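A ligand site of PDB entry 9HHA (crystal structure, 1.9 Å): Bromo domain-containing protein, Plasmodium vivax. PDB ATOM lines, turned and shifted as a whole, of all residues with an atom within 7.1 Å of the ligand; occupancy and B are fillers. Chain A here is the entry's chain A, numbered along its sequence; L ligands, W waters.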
ATOM      1  N   GLY A  22      27.589   9.480   8.562  1.00  0.00           N
ATOM      2  CA  GLY A  22      26.430   9.472   7.708  1.00  0.00           C
ATOM      3  C   GLY A  22      25.982   8.105   7.234  1.00  0.00           C
ATOM      4  O   GLY A  22      24.949   8.007   6.553  1.00  0.00           O
ATOM      5  N   HIS A  24      24.445   5.814   8.639  1.00  0.00           N
ATOM      6  CA  HIS A  24      23.165   5.361   9.152  1.00  0.00           C
ATOM      7  C   HIS A  24      22.049   5.447   8.120  1.00  0.00           C
ATOM      8  O   HIS A  24      21.062   4.707   8.223  1.00  0.00           O
ATOM      9  CB  HIS A  24      22.788   6.158  10.406  1.00  0.00           C
ATOM     10  CG  HIS A  24      22.524   7.605  10.130  1.00  0.00           C
ATOM     11  ND1 HIS A  24      23.530   8.544  10.001  1.00  0.00           N
ATOM     12  CD2 HIS A  24      21.363   8.275   9.945  1.00  0.00           C
ATOM     13  CE1 HIS A  24      22.997   9.723   9.753  1.00  0.00           C
ATOM     14  NE2 HIS A  24      21.688   9.586   9.720  1.00  0.00           N
ATOM     15  N   ILE A  25      22.187   6.318   7.113  1.00  0.00           N
ATOM     16  CA  ILE A  25      21.130   6.454   6.121  1.00  0.00           C
ATOM     17  C   ILE A  25      21.032   5.231   5.217  1.00  0.00           C
ATOM     18  O   ILE A  25      20.030   5.051   4.529  1.00  0.00           O
ATOM     19  CB  ILE A  25      21.311   7.725   5.274  1.00  0.00           C
ATOM     20  CG1 ILE A  25      22.496   7.578   4.317  1.00  0.00           C
ATOM     21  CG2 ILE A  25      21.490   8.948   6.180  1.00  0.00           C
ATOM     22  CD1 ILE A  25      22.622   8.730   3.323  1.00  0.00           C
ATOM     23  N   PHE A  26      22.069   4.386   5.200  1.00  0.00           N
ATOM     24  CA  PHE A  26      22.048   3.140   4.428  1.00  0.00           C
ATOM     25  C   PHE A  26      21.846   1.913   5.300  1.00  0.00           C
ATOM     26  O   PHE A  26      21.837   0.790   4.782  1.00  0.00           O
ATOM     27  CB  PHE A  26      23.349   2.983   3.629  1.00  0.00           C
ATOM     28  CG  PHE A  26      23.642   4.138   2.724  1.00  0.00           C
ATOM     29  CD1 PHE A  26      22.858   4.376   1.603  1.00  0.00           C
ATOM     30  CD2 PHE A  26      24.710   4.988   2.979  1.00  0.00           C
ATOM     31  CE1 PHE A  26      23.130   5.445   0.763  1.00  0.00           C
ATOM     32  CE2 PHE A  26      24.992   6.057   2.138  1.00  0.00           C
ATOM     33  CZ  PHE A  26      24.197   6.289   1.037  1.00  0.00           C
ATOM     34  N   GLU A  27      21.682   2.088   6.617  1.00  0.00           N
ATOM     35  CA  GLU A  27      21.629   0.938   7.519  1.00  0.00           C
ATOM     36  C   GLU A  27      20.370   0.111   7.310  1.00  0.00           C
ATOM     37  O   GLU A  27      20.431  -1.121   7.264  1.00  0.00           O
ATOM     38  CB  GLU A  27      21.720   1.408   8.976  1.00  0.00           C
ATOM     39  CG  GLU A  27      21.854   0.267   9.980  1.00  0.00           C
ATOM     40  CD  GLU A  27      23.173  -0.461   9.851  1.00  0.00           C
ATOM     41  OE1 GLU A  27      24.168   0.188   9.463  1.00  0.00           O
ATOM     42  OE2 GLU A  27      23.216  -1.678  10.128  1.00  0.00           O
ATOM     43  N   LYS A  28      19.227   0.768   7.195  1.00  0.00           N
ATOM     44  CA  LYS A  28      17.947   0.092   7.007  1.00  0.00           C
ATOM     45  C   LYS A  28      17.367   0.449   5.646  1.00  0.00           C
ATOM     46  O   LYS A  28      17.745   1.443   5.026  1.00  0.00           O
ATOM     47  CB  LYS A  28      16.947   0.466   8.110  1.00  0.00           C
ATOM     48  CG  LYS A  28      17.464   0.256   9.531  1.00  0.00           C
ATOM     49  CD  LYS A  28      17.657  -1.207   9.853  1.00  0.00           C
ATOM     50  CE  LYS A  28      18.053  -1.390  11.312  1.00  0.00           C
ATOM     51  NZ  LYS A  28      18.275  -2.822  11.667  1.00  0.00           N
ATOM     52  N   LEU A  29      16.435  -0.391   5.186  1.00  0.00           N
ATOM     53  CA  LEU A  29      15.733  -0.109   3.945  1.00  0.00           C
ATOM     54  C   LEU A  29      14.899   1.157   4.102  1.00  0.00           C
ATOM     55  O   LEU A  29      14.370   1.452   5.178  1.00  0.00           O
ATOM     56  CB  LEU A  29      14.841  -1.291   3.557  1.00  0.00           C
ATOM     57  CG  LEU A  29      15.592  -2.541   3.108  1.00  0.00           C
ATOM     58  CD1 LEU A  29      14.700  -3.770   3.159  1.00  0.00           C
ATOM     59  CD2 LEU A  29      16.165  -2.342   1.707  1.00  0.00           C
ATOM     60  N   VAL A  30      14.809   1.925   3.012  1.00  0.00           N
ATOM     61  CA  VAL A  30      14.079   3.194   3.045  1.00  0.00           C
ATOM     62  C   VAL A  30      12.613   2.932   3.335  1.00  0.00           C
ATOM     63  O   VAL A  30      11.984   2.052   2.729  1.00  0.00           O
ATOM     64  CB  VAL A  30      14.265   3.945   1.711  1.00  0.00           C
ATOM     65  CG1 VAL A  30      13.289   5.087   1.610  1.00  0.00           C
ATOM     66  CG2 VAL A  30      15.695   4.436   1.584  1.00  0.00           C
ATOM     67  N   ASP A  31      12.054   3.687   4.273  1.00  0.00           N
ATOM     68  CA  ASP A  31      10.618   3.701   4.501  1.00  0.00           C
ATOM     69  C   ASP A  31      10.040   4.811   3.624  1.00  0.00           C
ATOM     70  O   ASP A  31      10.214   5.995   3.912  1.00  0.00           O
ATOM     71  CB  ASP A  31      10.300   3.933   5.983  1.00  0.00           C
ATOM     72  CG  ASP A  31       8.823   3.725   6.302  1.00  0.00           C
ATOM     73  OD1 ASP A  31       7.957   4.224   5.556  1.00  0.00           O
ATOM     74  OD2 ASP A  31       8.543   3.068   7.327  1.00  0.00           O
ATOM     75  N   GLN A  35      10.115   8.563   5.110  1.00  0.00           N
ATOM     76  CA  GLN A  35      11.172   9.395   4.564  1.00  0.00           C
ATOM     77  C   GLN A  35      10.671  10.353   3.488  1.00  0.00           C
ATOM     78  O   GLN A  35      11.483  10.990   2.817  1.00  0.00           O
ATOM     79  CB  GLN A  35      12.303   8.528   4.001  1.00  0.00           C
ATOM     80  CG  GLN A  35      12.995   7.661   5.039  1.00  0.00           C
ATOM     81  CD  GLN A  35      13.560   8.477   6.192  1.00  0.00           C
ATOM     82  OE1 GLN A  35      13.935   9.639   6.032  1.00  0.00           O
ATOM     83  NE2 GLN A  35      13.606   7.864   7.378  1.00  0.00           N
ATOM     84  N   ASN A  36       9.355  10.449   3.302  1.00  0.00           N
ATOM     85  CA  ASN A  36       8.740  11.382   2.353  1.00  0.00           C
ATOM     86  C   ASN A  36       9.257  11.176   0.927  1.00  0.00           C
ATOM     87  O   ASN A  36       9.518  12.124   0.192  1.00  0.00           O
ATOM     88  CB  ASN A  36       8.948  12.830   2.797  1.00  0.00           C
ATOM     89  CG  ASN A  36       8.362  13.093   4.178  1.00  0.00           C
ATOM     90  OD1 ASN A  36       7.138  13.062   4.363  1.00  0.00           O
ATOM     91  ND2 ASN A  36       9.217  13.372   5.151  1.00  0.00           N
ATOM     92  N   CYS A  37       9.407   9.911   0.522  1.00  0.00           N
ATOM     93  CA  CYS A  37       9.773   9.555  -0.843  1.00  0.00           C
ATOM     94  C   CYS A  37       8.823   8.452  -1.310  1.00  0.00           C
ATOM     95  O   CYS A  37       9.226   7.297  -1.502  1.00  0.00           O
ATOM     96  CB  CYS A  37      11.239   9.125  -0.939  1.00  0.00           C
ATOM     97  SG  CYS A  37      11.778   7.969   0.312  1.00  0.00           S
ATOM     98  N   TYR A  40       9.811   5.895  -4.083  1.00  0.00           N
ATOM     99  CA  TYR A  40      11.134   5.297  -4.008  1.00  0.00           C
ATOM    100  C   TYR A  40      11.150   3.904  -4.629  1.00  0.00           C
ATOM    101  O   TYR A  40      12.052   3.573  -5.402  1.00  0.00           O
ATOM    102  CB  TYR A  40      11.609   5.232  -2.548  1.00  0.00           C
ATOM    103  CG  TYR A  40      13.000   4.666  -2.408  1.00  0.00           C
ATOM    104  CD1 TYR A  40      14.128   5.471  -2.569  1.00  0.00           C
ATOM    105  CD2 TYR A  40      13.194   3.320  -2.119  1.00  0.00           C
ATOM    106  CE1 TYR A  40      15.400   4.939  -2.441  1.00  0.00           C
ATOM    107  CE2 TYR A  40      14.465   2.778  -1.994  1.00  0.00           C
ATOM    108  CZ  TYR A  40      15.563   3.605  -2.159  1.00  0.00           C
ATOM    109  OH  TYR A  40      16.825   3.060  -2.024  1.00  0.00           O
ATOM    110  N   ILE A  44      13.442   2.246  -7.432  1.00  0.00           N
ATOM    111  CA  ILE A  44      14.438   1.293  -6.958  1.00  0.00           C
ATOM    112  C   ILE A  44      13.767  -0.079  -6.909  1.00  0.00           C
ATOM    113  O   ILE A  44      12.967  -0.363  -6.008  1.00  0.00           O
ATOM    114  CB  ILE A  44      15.002   1.695  -5.588  1.00  0.00           C
ATOM    115  CG1 ILE A  44      15.694   3.062  -5.680  1.00  0.00           C
ATOM    116  CG2 ILE A  44      15.968   0.637  -5.087  1.00  0.00           C
ATOM    117  CD1 ILE A  44      16.672   3.172  -6.838  1.00  0.00           C
ATOM    118  N   MET A  48      18.447  -2.393  -1.183  1.00  0.00           N
ATOM    119  CA  MET A  48      19.493  -3.030  -0.397  1.00  0.00           C
ATOM    120  C   MET A  48      19.949  -2.065   0.689  1.00  0.00           C
ATOM    121  O   MET A  48      19.964  -0.851   0.486  1.00  0.00           O
ATOM    122  CB  MET A  48      20.678  -3.442  -1.288  1.00  0.00           C
ATOM    123  CG  MET A  48      21.738  -4.299  -0.599  1.00  0.00           C
ATOM    124  SD  MET A  48      21.097  -5.902  -0.068  1.00  0.00           S
ATOM    125  CE  MET A  48      20.510  -6.583  -1.609  1.00  0.00           C
ATOM    126  N   ILE A  75      23.764  -0.852  -3.116  1.00  0.00           N
ATOM    127  CA  ILE A  75      23.324   0.231  -2.230  1.00  0.00           C
ATOM    128  C   ILE A  75      23.698   1.576  -2.824  1.00  0.00           C
ATOM    129  O   ILE A  75      22.872   2.500  -2.903  1.00  0.00           O
ATOM    130  CB  ILE A  75      23.931   0.051  -0.829  1.00  0.00           C
ATOM    131  CG1 ILE A  75      23.536  -1.298  -0.226  1.00  0.00           C
ATOM    132  CG2 ILE A  75      23.489   1.193   0.098  1.00  0.00           C
ATOM    133  CD1 ILE A  75      24.186  -1.543   1.122  1.00  0.00           C
ATOM    134  N   ASN A  78      21.824   2.333  -6.192  1.00  0.00           N
ATOM    135  CA  ASN A  78      20.472   2.799  -5.890  1.00  0.00           C
ATOM    136  C   ASN A  78      20.490   4.245  -5.419  1.00  0.00           C
ATOM    137  O   ASN A  78      19.633   5.046  -5.816  1.00  0.00           O
ATOM    138  CB  ASN A  78      19.813   1.911  -4.826  1.00  0.00           C
ATOM    139  CG  ASN A  78      19.447   0.545  -5.361  1.00  0.00           C
ATOM    140  OD1 ASN A  78      19.348   0.347  -6.565  1.00  0.00           O
ATOM    141  ND2 ASN A  78      19.231  -0.401  -4.445  1.00  0.00           N
ATOM    142  N   CYS A  79      21.446   4.587  -4.559  1.00  0.00           N
ATOM    143  CA  CYS A  79      21.543   5.941  -4.034  1.00  0.00           C
ATOM    144  C   CYS A  79      21.733   6.959  -5.158  1.00  0.00           C
ATOM    145  O   CYS A  79      21.026   7.966  -5.226  1.00  0.00           O
ATOM    146  CB  CYS A  79      22.688   6.020  -3.018  1.00  0.00           C
ATOM    147  SG  CYS A  79      22.928   7.680  -2.330  1.00  0.00           S
ATOM    148  N   SER A  80      22.687   6.699  -6.043  1.00  0.00           N
ATOM    149  CA  SER A  80      22.956   7.641  -7.129  1.00  0.00           C
ATOM    150  C   SER A  80      21.810   7.680  -8.146  1.00  0.00           C
ATOM    151  O   SER A  80      21.578   8.720  -8.775  1.00  0.00           O
ATOM    152  CB  SER A  80      24.276   7.287  -7.816  1.00  0.00           C
ATOM    153  OG  SER A  80      24.210   5.987  -8.375  1.00  0.00           O
ATOM    154  N   TYR A  82      18.426   7.198  -7.466  1.00  0.00           N
ATOM    155  CA  TYR A  82      17.248   7.903  -6.961  1.00  0.00           C
ATOM    156  C   TYR A  82      17.550   9.360  -6.660  1.00  0.00           C
ATOM    157  O   TYR A  82      16.719  10.242  -6.922  1.00  0.00           O
ATOM    158  CB  TYR A  82      16.693   7.210  -5.721  1.00  0.00           C
ATOM    159  CG  TYR A  82      15.416   7.861  -5.247  1.00  0.00           C
ATOM    160  CD1 TYR A  82      14.203   7.552  -5.847  1.00  0.00           C
ATOM    161  CD2 TYR A  82      15.424   8.810  -4.229  1.00  0.00           C
ATOM    162  CE1 TYR A  82      13.027   8.151  -5.432  1.00  0.00           C
ATOM    163  CE2 TYR A  82      14.248   9.415  -3.801  1.00  0.00           C
ATOM    164  CZ  TYR A  82      13.055   9.078  -4.410  1.00  0.00           C
ATOM    165  OH  TYR A  82      11.890   9.680  -4.004  1.00  0.00           O
ATOM    166  N   ASN A  83      18.713   9.653  -6.078  1.00  0.00           N
ATOM    167  CA  ASN A  83      19.000  10.968  -5.551  1.00  0.00           C
ATOM    168  C   ASN A  83      19.769  11.824  -6.550  1.00  0.00           C
ATOM    169  O   ASN A  83      20.679  11.344  -7.226  1.00  0.00           O
ATOM    170  CB  ASN A  83      19.799  10.854  -4.239  1.00  0.00           C
ATOM    171  CG  ASN A  83      19.039  10.085  -3.189  1.00  0.00           C
ATOM    172  OD1 ASN A  83      18.149  10.639  -2.539  1.00  0.00           O
ATOM    173  ND2 ASN A  83      19.356   8.808  -3.033  1.00  0.00           N
ATOM    174  N   LEU A  88      22.397  16.033  -0.435  1.00  0.00           N
ATOM    175  CA  LEU A  88      23.052  15.530   0.771  1.00  0.00           C
ATOM    176  C   LEU A  88      23.174  14.010   0.732  1.00  0.00           C
ATOM    177  O   LEU A  88      24.241  13.458   1.061  1.00  0.00           O
ATOM    178  CB  LEU A  88      22.278  15.942   2.019  1.00  0.00           C
ATOM    179  CG  LEU A  88      22.561  17.286   2.672  1.00  0.00           C
ATOM    180  CD1 LEU A  88      22.036  17.277   4.108  1.00  0.00           C
ATOM    181  CD2 LEU A  88      24.050  17.605   2.646  1.00  0.00           C
ATOM    182  N   VAL A  89      22.109  13.314   0.340  1.00  0.00           N
ATOM    183  CA  VAL A  89      22.141  11.860   0.323  1.00  0.00           C
ATOM    184  C   VAL A  89      23.101  11.356  -0.742  1.00  0.00           C
ATOM    185  O   VAL A  89      23.902  10.445  -0.490  1.00  0.00           O
ATOM    186  CB  VAL A  89      20.710  11.307   0.110  1.00  0.00           C
ATOM    187  CG1 VAL A  89      20.758   9.805  -0.167  1.00  0.00           C
ATOM    188  CG2 VAL A  89      19.857  11.585   1.342  1.00  0.00           C
ATOM    189  N   THR A  92      26.692  11.740   0.391  1.00  0.00           N
ATOM    190  CA  THR A  92      27.045  10.735   1.384  1.00  0.00           C
ATOM    191  C   THR A  92      27.312   9.379   0.728  1.00  0.00           C
ATOM    192  O   THR A  92      28.259   8.677   1.087  1.00  0.00           O
ATOM    193  CB  THR A  92      25.940  10.618   2.431  1.00  0.00           C
ATOM    194  OG1 THR A  92      25.725  11.909   3.033  1.00  0.00           O
ATOM    195  CG2 THR A  92      26.321   9.612   3.519  1.00  0.00           C
HETATM  196  C1  LIG L   1      16.918   6.742   5.673  1.00  0.00           C
HETATM  197  C2  LIG L   1      17.575   7.590   3.473  1.00  0.00           C
HETATM  198  C3  LIG L   1      19.661   5.899   0.940  1.00  0.00           C
HETATM  199  C4  LIG L   1      15.665   8.909   2.238  1.00  0.00           C
HETATM  200  C5  LIG L   1      15.844  10.227   1.439  1.00  0.00           C
HETATM  201  C6  LIG L   1      16.042  10.038  -0.051  1.00  0.00           C
HETATM  202  C7  LIG L   1      15.874   8.587  -0.485  1.00  0.00           C
HETATM  203  C8  LIG L   1      17.083   7.726  -0.175  1.00  0.00           C
HETATM  204  C9  LIG L   1      17.542   7.470   1.196  1.00  0.00           C
HETATM  205  C10 LIG L   1      16.879   8.032   2.351  1.00  0.00           C
HETATM  206  C11 LIG L   1      18.627   6.704   1.653  1.00  0.00           C
HETATM  207  C12 LIG L   1      17.368   7.818   4.913  1.00  0.00           C
HETATM  208  C13 LIG L   1      16.703   6.843   7.049  1.00  0.00           C
HETATM  209  C14 LIG L   1      16.948   8.042   7.693  1.00  0.00           C
HETATM  210  C15 LIG L   1      17.408   9.140   6.962  1.00  0.00           C
HETATM  211  C16 LIG L   1      17.622   9.029   5.583  1.00  0.00           C
HETATM  212  C17 LIG L   1      18.130  10.291   4.868  1.00  0.00           C
HETATM  213  F1  LIG L   1      18.654  11.228   5.671  1.00  0.00           F
HETATM  214  F2  LIG L   1      17.192  10.931   4.170  1.00  0.00           F
HETATM  215  F3  LIG L   1      19.114  10.010   3.987  1.00  0.00           F
HETATM  216  N1  LIG L   1      18.632   6.782   3.046  1.00  0.00           N
HETATM  217  O1  LIG L   1      17.690   7.227  -1.119  1.00  0.00           O
HETATM  218  O   HOH W   1      18.868   4.877  -2.312  1.00  0.00           O
HETATM  219  O   HOH W   2      16.245   3.750   6.303  1.00  0.00           O
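Water W1 lies within hydrogen-bond range of the side-chain hydroxyl (OH) of Tyr 40 (2.7 Å), an oxygen (O1) of the ligand (2.9 Å) and the backbone NH (N) of Cys 79 (3.4 Å).
O of Val 89 sits at hydrogen-bond distance from SG of Cys 79, at 3.5 Å. ND2 of Asn 83 is in hydrogen-bond range of O of Cys 79 (2.9 Å).
N1 of the ligand is in hydrogen-bond range of O of Ile 25. ND2 of Asn 83 lies within hydrogen-bond range of O1 of the ligand, 3.0 Å away.
Phe 26 touches the ligand. Val 30 touches the ligand (CG2 to C9, 3.6 Å). NE2 of Gln 35 touches C13 of the ligand (3.3 Å). Tyr 40 touches the ligand (CE1 to O1, 3.5 Å). Tyr 82 touches the ligand (CD2 to C7, 3.8 Å). CG2 of Val 89 touches F3 of the ligand (3.2 Å). Hydrophobic or aromatic side chains that line the ligand: Ile 25, Phe 26, Val 30, Tyr 40, Tyr 82 and Val 89. Eight residues have an atom within 4 Å of the ligand: Ile 25, Phe 26, Val 30, Gln 35, Tyr 40, Tyr 82, Asn 83 and Val 89.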
